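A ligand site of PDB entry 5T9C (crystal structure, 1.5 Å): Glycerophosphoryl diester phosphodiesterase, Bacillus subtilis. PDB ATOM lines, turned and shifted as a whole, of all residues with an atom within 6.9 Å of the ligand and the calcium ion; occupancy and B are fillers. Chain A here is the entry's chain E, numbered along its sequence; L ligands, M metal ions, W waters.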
ATOM      1  N   HIS A  18      12.822   2.983 -23.354  1.00  0.00           N
ATOM      2  CA  HIS A  18      11.657   2.748 -22.498  1.00  0.00           C
ATOM      3  C   HIS A  18      11.945   3.069 -21.037  1.00  0.00           C
ATOM      4  O   HIS A  18      12.639   2.318 -20.354  1.00  0.00           O
ATOM      5  CB  HIS A  18      11.257   1.283 -22.652  1.00  0.00           C
ATOM      6  CG  HIS A  18      10.016   0.890 -21.913  1.00  0.00           C
ATOM      7  ND1 HIS A  18      10.018  -0.089 -20.940  1.00  0.00           N
ATOM      8  CD2 HIS A  18       8.734   1.333 -22.010  1.00  0.00           C
ATOM      9  CE1 HIS A  18       8.779  -0.241 -20.479  1.00  0.00           C
ATOM     10  NE2 HIS A  18       7.994   0.612 -21.109  1.00  0.00           N
ATOM     11  N   ARG A  19      11.392   4.191 -20.552  1.00  0.00           N
ATOM     12  CA  ARG A  19      11.652   4.679 -19.191  1.00  0.00           C
ATOM     13  C   ARG A  19      13.144   4.943 -18.991  1.00  0.00           C
ATOM     14  O   ARG A  19      13.672   4.815 -17.890  1.00  0.00           O
ATOM     15  CB  ARG A  19      11.108   3.693 -18.149  1.00  0.00           C
ATOM     16  CG  ARG A  19       9.731   3.089 -18.530  1.00  0.00           C
ATOM     17  CD  ARG A  19       9.099   2.249 -17.428  1.00  0.00           C
ATOM     18  NE  ARG A  19       7.921   1.559 -17.941  1.00  0.00           N
ATOM     19  CZ  ARG A  19       7.313   0.536 -17.337  1.00  0.00           C
ATOM     20  NH1 ARG A  19       7.748   0.093 -16.168  1.00  0.00           N
ATOM     21  NH2 ARG A  19       6.276  -0.061 -17.909  1.00  0.00           N
ATOM     22  N   HIS A  28      12.754   5.819 -15.124  1.00  0.00           N
ATOM     23  CA  HIS A  28      12.238   7.178 -14.923  1.00  0.00           C
ATOM     24  C   HIS A  28      13.000   7.933 -13.840  1.00  0.00           C
ATOM     25  O   HIS A  28      12.394   8.608 -12.999  1.00  0.00           O
ATOM     26  CB  HIS A  28      10.751   7.126 -14.582  1.00  0.00           C
ATOM     27  CG  HIS A  28       9.881   6.671 -15.721  1.00  0.00           C
ATOM     28  ND1 HIS A  28      10.100   7.060 -17.027  1.00  0.00           N
ATOM     29  CD2 HIS A  28       8.784   5.888 -15.734  1.00  0.00           C
ATOM     30  CE1 HIS A  28       9.158   6.539 -17.794  1.00  0.00           C
ATOM     31  NE2 HIS A  28       8.345   5.819 -17.039  1.00  0.00           N
ATOM     32  N   GLU A  45      11.988   8.052 -23.069  1.00  0.00           N
ATOM     33  CA  GLU A  45      10.552   7.845 -22.932  1.00  0.00           C
ATOM     34  C   GLU A  45      10.068   8.095 -21.510  1.00  0.00           C
ATOM     35  O   GLU A  45      10.609   7.548 -20.549  1.00  0.00           O
ATOM     36  CB  GLU A  45      10.198   6.412 -23.384  1.00  0.00           C
ATOM     37  CG  GLU A  45       8.708   6.209 -23.634  1.00  0.00           C
ATOM     38  CD  GLU A  45       8.015   5.391 -22.561  1.00  0.00           C
ATOM     39  OE1 GLU A  45       8.683   4.815 -21.668  1.00  0.00           O
ATOM     40  OE2 GLU A  45       6.767   5.319 -22.601  1.00  0.00           O
ATOM     41  N   LEU A  46       9.051   8.953 -21.394  1.00  0.00           N
ATOM     42  CA  LEU A  46       8.508   9.379 -20.119  1.00  0.00           C
ATOM     43  C   LEU A  46       7.056   8.948 -19.980  1.00  0.00           C
ATOM     44  O   LEU A  46       6.319   9.027 -20.953  1.00  0.00           O
ATOM     45  CB  LEU A  46       8.571  10.903 -19.985  1.00  0.00           C
ATOM     46  CG  LEU A  46       9.912  11.592 -19.717  1.00  0.00           C
ATOM     47  CD1 LEU A  46      11.001  11.288 -20.747  1.00  0.00           C
ATOM     48  CD2 LEU A  46       9.615  13.092 -19.703  1.00  0.00           C
ATOM     49  N   ASP A  47       6.659   8.539 -18.777  1.00  0.00           N
ATOM     50  CA  ASP A  47       5.249   8.325 -18.426  1.00  0.00           C
ATOM     51  C   ASP A  47       4.861   9.412 -17.435  1.00  0.00           C
ATOM     52  O   ASP A  47       5.589   9.616 -16.459  1.00  0.00           O
ATOM     53  CB  ASP A  47       5.010   6.956 -17.798  1.00  0.00           C
ATOM     54  CG  ASP A  47       5.346   5.794 -18.707  1.00  0.00           C
ATOM     55  OD1 ASP A  47       4.912   5.767 -19.896  1.00  0.00           O
ATOM     56  OD2 ASP A  47       6.017   4.878 -18.204  1.00  0.00           O
ATOM     57  N   HIS A  60       5.661   5.598 -14.004  1.00  0.00           N
ATOM     58  CA  HIS A  60       4.803   4.727 -14.811  1.00  0.00           C
ATOM     59  C   HIS A  60       3.458   4.447 -14.156  1.00  0.00           C
ATOM     60  O   HIS A  60       2.411   4.572 -14.795  1.00  0.00           O
ATOM     61  CB  HIS A  60       5.479   3.400 -15.123  1.00  0.00           C
ATOM     62  CG  HIS A  60       4.579   2.454 -15.838  1.00  0.00           C
ATOM     63  ND1 HIS A  60       3.773   1.552 -15.174  1.00  0.00           N
ATOM     64  CD2 HIS A  60       4.298   2.318 -17.153  1.00  0.00           C
ATOM     65  CE1 HIS A  60       3.061   0.867 -16.055  1.00  0.00           C
ATOM     66  NE2 HIS A  60       3.364   1.320 -17.264  1.00  0.00           N
ATOM     67  N   TYR A 125       9.719  11.292 -25.776  1.00  0.00           N
ATOM     68  CA  TYR A 125       8.578  10.460 -26.157  1.00  0.00           C
ATOM     69  C   TYR A 125       7.704  10.361 -24.929  1.00  0.00           C
ATOM     70  O   TYR A 125       8.023   9.624 -24.009  1.00  0.00           O
ATOM     71  CB  TYR A 125       9.080   9.087 -26.616  1.00  0.00           C
ATOM     72  CG  TYR A 125       8.280   8.398 -27.698  1.00  0.00           C
ATOM     73  CD1 TYR A 125       8.891   7.967 -28.872  1.00  0.00           C
ATOM     74  CD2 TYR A 125       6.916   8.172 -27.554  1.00  0.00           C
ATOM     75  CE1 TYR A 125       8.192   7.302 -29.855  1.00  0.00           C
ATOM     76  CE2 TYR A 125       6.194   7.511 -28.544  1.00  0.00           C
ATOM     77  CZ  TYR A 125       6.835   7.080 -29.688  1.00  0.00           C
ATOM     78  OH  TYR A 125       6.110   6.423 -30.665  1.00  0.00           O
ATOM     79  N   GLU A 127       4.301   9.982 -22.577  1.00  0.00           N
ATOM     80  CA  GLU A 127       2.973   9.383 -22.446  1.00  0.00           C
ATOM     81  C   GLU A 127       2.104  10.040 -21.391  1.00  0.00           C
ATOM     82  O   GLU A 127       2.535  10.275 -20.265  1.00  0.00           O
ATOM     83  CB  GLU A 127       3.093   7.892 -22.122  1.00  0.00           C
ATOM     84  CG  GLU A 127       1.724   7.191 -22.141  1.00  0.00           C
ATOM     85  CD  GLU A 127       1.827   5.691 -21.940  1.00  0.00           C
ATOM     86  OE1 GLU A 127       2.943   5.132 -22.109  1.00  0.00           O
ATOM     87  OE2 GLU A 127       0.778   5.090 -21.638  1.00  0.00           O
ATOM     88  N   LYS A 129      -0.534   9.284 -18.923  1.00  0.00           N
ATOM     89  CA  LYS A 129      -1.144   8.164 -18.218  1.00  0.00           C
ATOM     90  C   LYS A 129      -2.440   8.577 -17.561  1.00  0.00           C
ATOM     91  O   LYS A 129      -2.524   9.649 -16.975  1.00  0.00           O
ATOM     92  CB  LYS A 129      -0.209   7.611 -17.142  1.00  0.00           C
ATOM     93  CG  LYS A 129       1.011   6.880 -17.680  1.00  0.00           C
ATOM     94  CD  LYS A 129       0.620   5.564 -18.362  1.00  0.00           C
ATOM     95  CE  LYS A 129       1.880   4.765 -18.670  1.00  0.00           C
ATOM     96  NZ  LYS A 129       1.572   3.538 -19.485  1.00  0.00           N
ATOM     97  N   GLN A 163       2.336  10.391 -26.722  1.00  0.00           N
ATOM     98  CA  GLN A 163       1.749   9.070 -26.906  1.00  0.00           C
ATOM     99  C   GLN A 163       0.758   8.805 -25.795  1.00  0.00           C
ATOM    100  O   GLN A 163       0.848   9.401 -24.721  1.00  0.00           O
ATOM    101  CB  GLN A 163       2.844   7.999 -26.903  1.00  0.00           C
ATOM    102  CG  GLN A 163       3.803   8.206 -25.738  1.00  0.00           C
ATOM    103  CD  GLN A 163       4.595   6.974 -25.362  1.00  0.00           C
ATOM    104  OE1 GLN A 163       4.361   5.871 -25.888  1.00  0.00           O
ATOM    105  NE2 GLN A 163       5.558   7.148 -24.452  1.00  0.00           N
ATOM    106  N   SER A 164      -0.195   7.908 -26.035  1.00  0.00           N
ATOM    107  CA  SER A 164      -1.156   7.559 -24.995  1.00  0.00           C
ATOM    108  C   SER A 164      -1.958   6.344 -25.454  1.00  0.00           C
ATOM    109  O   SER A 164      -2.142   6.134 -26.646  1.00  0.00           O
ATOM    110  CB  SER A 164      -2.110   8.724 -24.708  1.00  0.00           C
ATOM    111  OG  SER A 164      -2.886   8.506 -23.540  1.00  0.00           O
ATOM    112  N   PHE A 165      -2.448   5.584 -24.483  1.00  0.00           N
ATOM    113  CA  PHE A 165      -3.515   4.628 -24.760  1.00  0.00           C
ATOM    114  C   PHE A 165      -4.854   5.337 -24.966  1.00  0.00           C
ATOM    115  O   PHE A 165      -5.754   4.796 -25.625  1.00  0.00           O
ATOM    116  CB  PHE A 165      -3.616   3.601 -23.634  1.00  0.00           C
ATOM    117  CG  PHE A 165      -2.508   2.586 -23.662  1.00  0.00           C
ATOM    118  CD1 PHE A 165      -2.585   1.487 -24.496  1.00  0.00           C
ATOM    119  CD2 PHE A 165      -1.386   2.742 -22.863  1.00  0.00           C
ATOM    120  CE1 PHE A 165      -1.543   0.552 -24.527  1.00  0.00           C
ATOM    121  CE2 PHE A 165      -0.361   1.820 -22.886  1.00  0.00           C
ATOM    122  CZ  PHE A 165      -0.428   0.724 -23.720  1.00  0.00           C
ATOM    123  N   LEU A 185      -1.117   4.358 -28.750  1.00  0.00           N
ATOM    124  CA  LEU A 185      -0.713   3.096 -28.155  1.00  0.00           C
ATOM    125  C   LEU A 185      -1.863   2.098 -28.170  1.00  0.00           C
ATOM    126  O   LEU A 185      -3.045   2.450 -28.009  1.00  0.00           O
ATOM    127  CB  LEU A 185      -0.213   3.304 -26.730  1.00  0.00           C
ATOM    128  CG  LEU A 185       0.968   4.275 -26.576  1.00  0.00           C
ATOM    129  CD1 LEU A 185       1.309   4.415 -25.111  1.00  0.00           C
ATOM    130  CD2 LEU A 185       2.169   3.753 -27.371  1.00  0.00           C
ATOM    131  N   GLY A 210       1.692   2.403 -31.728  1.00  0.00           N
ATOM    132  CA  GLY A 210       2.599   1.742 -30.806  1.00  0.00           C
ATOM    133  C   GLY A 210       1.903   0.554 -30.167  1.00  0.00           C
ATOM    134  O   GLY A 210       1.354   0.668 -29.072  1.00  0.00           O
ATOM    135  N   HIS A 232       5.945   1.634 -33.901  1.00  0.00           N
ATOM    136  CA  HIS A 232       6.869   1.540 -32.766  1.00  0.00           C
ATOM    137  C   HIS A 232       6.339   0.573 -31.728  1.00  0.00           C
ATOM    138  O   HIS A 232       5.677   0.990 -30.775  1.00  0.00           O
ATOM    139  CB  HIS A 232       7.064   2.915 -32.096  1.00  0.00           C
ATOM    140  CG  HIS A 232       7.638   3.956 -32.996  1.00  0.00           C
ATOM    141  ND1 HIS A 232       7.521   5.307 -32.724  1.00  0.00           N
ATOM    142  CD2 HIS A 232       8.357   3.861 -34.142  1.00  0.00           C
ATOM    143  CE1 HIS A 232       8.127   5.994 -33.683  1.00  0.00           C
ATOM    144  NE2 HIS A 232       8.645   5.142 -34.539  1.00  0.00           N
ATOM    145  N   PRO A 233       6.627  -0.716 -31.890  1.00  0.00           N
ATOM    146  CA  PRO A 233       6.073  -1.667 -30.909  1.00  0.00           C
ATOM    147  C   PRO A 233       6.816  -1.602 -29.579  1.00  0.00           C
ATOM    148  O   PRO A 233       7.988  -1.188 -29.547  1.00  0.00           O
ATOM    149  CB  PRO A 233       6.256  -3.033 -31.587  1.00  0.00           C
ATOM    150  CG  PRO A 233       7.279  -2.838 -32.623  1.00  0.00           C
ATOM    151  CD  PRO A 233       7.251  -1.392 -33.040  1.00  0.00           C
ATOM    152  N   TYR A 234       6.128  -1.987 -28.503  1.00  0.00           N
ATOM    153  CA  TYR A 234       6.681  -2.023 -27.145  1.00  0.00           C
ATOM    154  C   TYR A 234       6.426  -3.421 -26.571  1.00  0.00           C
ATOM    155  O   TYR A 234       5.534  -4.123 -27.061  1.00  0.00           O
ATOM    156  CB  TYR A 234       6.028  -0.961 -26.228  1.00  0.00           C
ATOM    157  CG  TYR A 234       4.562  -1.260 -25.954  1.00  0.00           C
ATOM    158  CD1 TYR A 234       4.188  -2.105 -24.920  1.00  0.00           C
ATOM    159  CD2 TYR A 234       3.561  -0.713 -26.753  1.00  0.00           C
ATOM    160  CE1 TYR A 234       2.849  -2.412 -24.682  1.00  0.00           C
ATOM    161  CE2 TYR A 234       2.226  -1.004 -26.519  1.00  0.00           C
ATOM    162  CZ  TYR A 234       1.870  -1.865 -25.484  1.00  0.00           C
ATOM    163  OH  TYR A 234       0.540  -2.169 -25.245  1.00  0.00           O
ATOM    164  N   THR A 235       7.178  -3.859 -25.560  1.00  0.00           N
ATOM    165  CA  THR A 235       8.517  -3.364 -25.213  1.00  0.00           C
ATOM    166  C   THR A 235       9.466  -4.497 -25.595  1.00  0.00           C
ATOM    167  O   THR A 235       9.323  -5.622 -25.110  1.00  0.00           O
ATOM    168  CB  THR A 235       8.637  -3.038 -23.723  1.00  0.00           C
ATOM    169  OG1 THR A 235       7.772  -1.937 -23.417  1.00  0.00           O
ATOM    170  CG2 THR A 235      10.085  -2.652 -23.367  1.00  0.00           C
ATOM    171  N   PHE A 254      10.216   0.553 -28.647  1.00  0.00           N
ATOM    172  CA  PHE A 254      10.466   0.874 -27.249  1.00  0.00           C
ATOM    173  C   PHE A 254      11.268  -0.274 -26.661  1.00  0.00           C
ATOM    174  O   PHE A 254      10.850  -1.443 -26.773  1.00  0.00           O
ATOM    175  CB  PHE A 254       9.165   1.056 -26.440  1.00  0.00           C
ATOM    176  CG  PHE A 254       8.249   2.143 -26.934  1.00  0.00           C
ATOM    177  CD1 PHE A 254       7.373   1.919 -27.982  1.00  0.00           C
ATOM    178  CD2 PHE A 254       8.228   3.394 -26.309  1.00  0.00           C
ATOM    179  CE1 PHE A 254       6.514   2.908 -28.415  1.00  0.00           C
ATOM    180  CE2 PHE A 254       7.365   4.391 -26.738  1.00  0.00           C
ATOM    181  CZ  PHE A 254       6.501   4.142 -27.798  1.00  0.00           C
HETATM  182  O1  LIG L   1       4.602   3.835 -24.280  1.00  0.00           O
HETATM  183  C1  LIG L   1       4.796   2.554 -24.879  1.00  0.00           C
HETATM  184  C2  LIG L   1       4.808   1.544 -23.755  1.00  0.00           C
HETATM  185  O2  LIG L   1       5.684   2.013 -22.742  1.00  0.00           O
HETATM  186  C3  LIG L   1       3.382   1.337 -23.258  1.00  0.00           C
HETATM  187  O3  LIG L   1       3.367   0.515 -22.104  1.00  0.00           O
HETATM  188  O4  LIG L   1       2.931   0.264 -19.635  1.00  0.00           O
HETATM  189  O5  LIG L   1       5.282   0.413 -20.482  1.00  0.00           O
HETATM  190  O6  LIG L   1       3.793   2.423 -20.544  1.00  0.00           O
HETATM  191  P1  LIG L   1       3.864   0.908 -20.642  1.00  0.00           P
HETATM  192 CA    CA M   1       4.982   4.131 -21.700  1.00  0.00          CA
HETATM  193  O   HOH W   1       5.924  -2.262 -21.444  1.00  0.00           O
HETATM  194  O   HOH W   2       6.908   3.377 -20.209  1.00  0.00           O
HETATM  195  O   HOH W   3       1.313  -1.926 -20.293  1.00  0.00           O
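Within 4 Å of the calcium ion: Glu 45, Asp 47 and Glu 127.
Along chain A the residues within 4 Å of the calcium ion span positions 45 to 127.
The nearest printed residue that does not touch the calcium ion is Lys 129 (4.1 Å).
The side-chain amide oxygen of Gln 163 sits close to an oxygen (O1) of the ligand, 2.6 Å away.
A ring nitrogen (NE2) of His 60 sits at hydrogen-bond distance from an oxygen (O4) of the ligand (2.6 Å).
NZ of Lys 129 is in salt-bridge range of O4 of the ligand, at 3.5 Å.
A ring nitrogen (NE2) of His 18 lies within hydrogen-bond range of an oxygen (O5) of the ligand (2.8 Å).
The guanidinium group (NH2) of Arg 19 lies within salt-bridge range of an oxygen (O5) of the ligand (2.8 Å).
CE2 of Phe 165 touches C3 of the ligand (3.8 Å).
Leu 185 touches the ligand.
Tyr 234 touches the ligand (CG to C2, 3.6 Å).
CE2 of Phe 254 touches C1 of the ligand, at 3.7 Å.
Hydrophobic or aromatic side chains within 4 Å of the ligand: His 18, His 60, Phe 165, Leu 185, Tyr 234 and Phe 254.
Along chain A the residues within 4 Å of the ligand span positions 18 to 254.
The calcium ion is bound by the side-chain carboxylate of Glu 127, the side-chain carboxylate of Glu 45, an oxygen (O6) of the ligand, the side-chain carboxylate of Asp 47, an oxygen (O2) of the ligand, water W2 and an oxygen (O1) of the ligand.
The calcium ion has seven donor atoms within binding distance.
Water W2 lies within hydrogen-bond range of the side-chain carboxylate of Asp 47, the side-chain carboxylate of Glu 45, the guanidinium group of Arg 19, a ring nitrogen (NE2) of His 18 and an oxygen (O5) of the ligand.
Water W1 lies within hydrogen-bond range of OG1 of Thr 235 (2.7 Å) and O5 of the ligand (2.9 Å).
The backbone NH of Glu 127 sits at hydrogen-bond distance from the backbone carbonyl oxygen of Leu 46 (2.8 Å).
The side-chain carboxylate of Glu 45 sits at hydrogen-bond distance from the backbone NH of Arg 19, at 3.0 Å.
OD2 of Asp 47 lies within salt-bridge range of NE of Arg 19 (3.8 Å).
OD2 of Asp 47 lies within hydrogen-bond range of NE2 of His 28, 2.8 Å away.
The guanidinium group (NH2) of Arg 19 sits close to a ring nitrogen (NE2) of His 60.
OG1 of Thr 235 lies within hydrogen-bond range of NE2 of His 18, 3.4 Å away.
The backbone carbonyl oxygen (O) of Arg 19 sits at hydrogen-bond distance from the backbone NH (N) of His 28 (3.1 Å).
The backbone carbonyl oxygen (O) of Ser 164 is in hydrogen-bond range of the backbone NH (N) of Leu 185 (2.9 Å).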
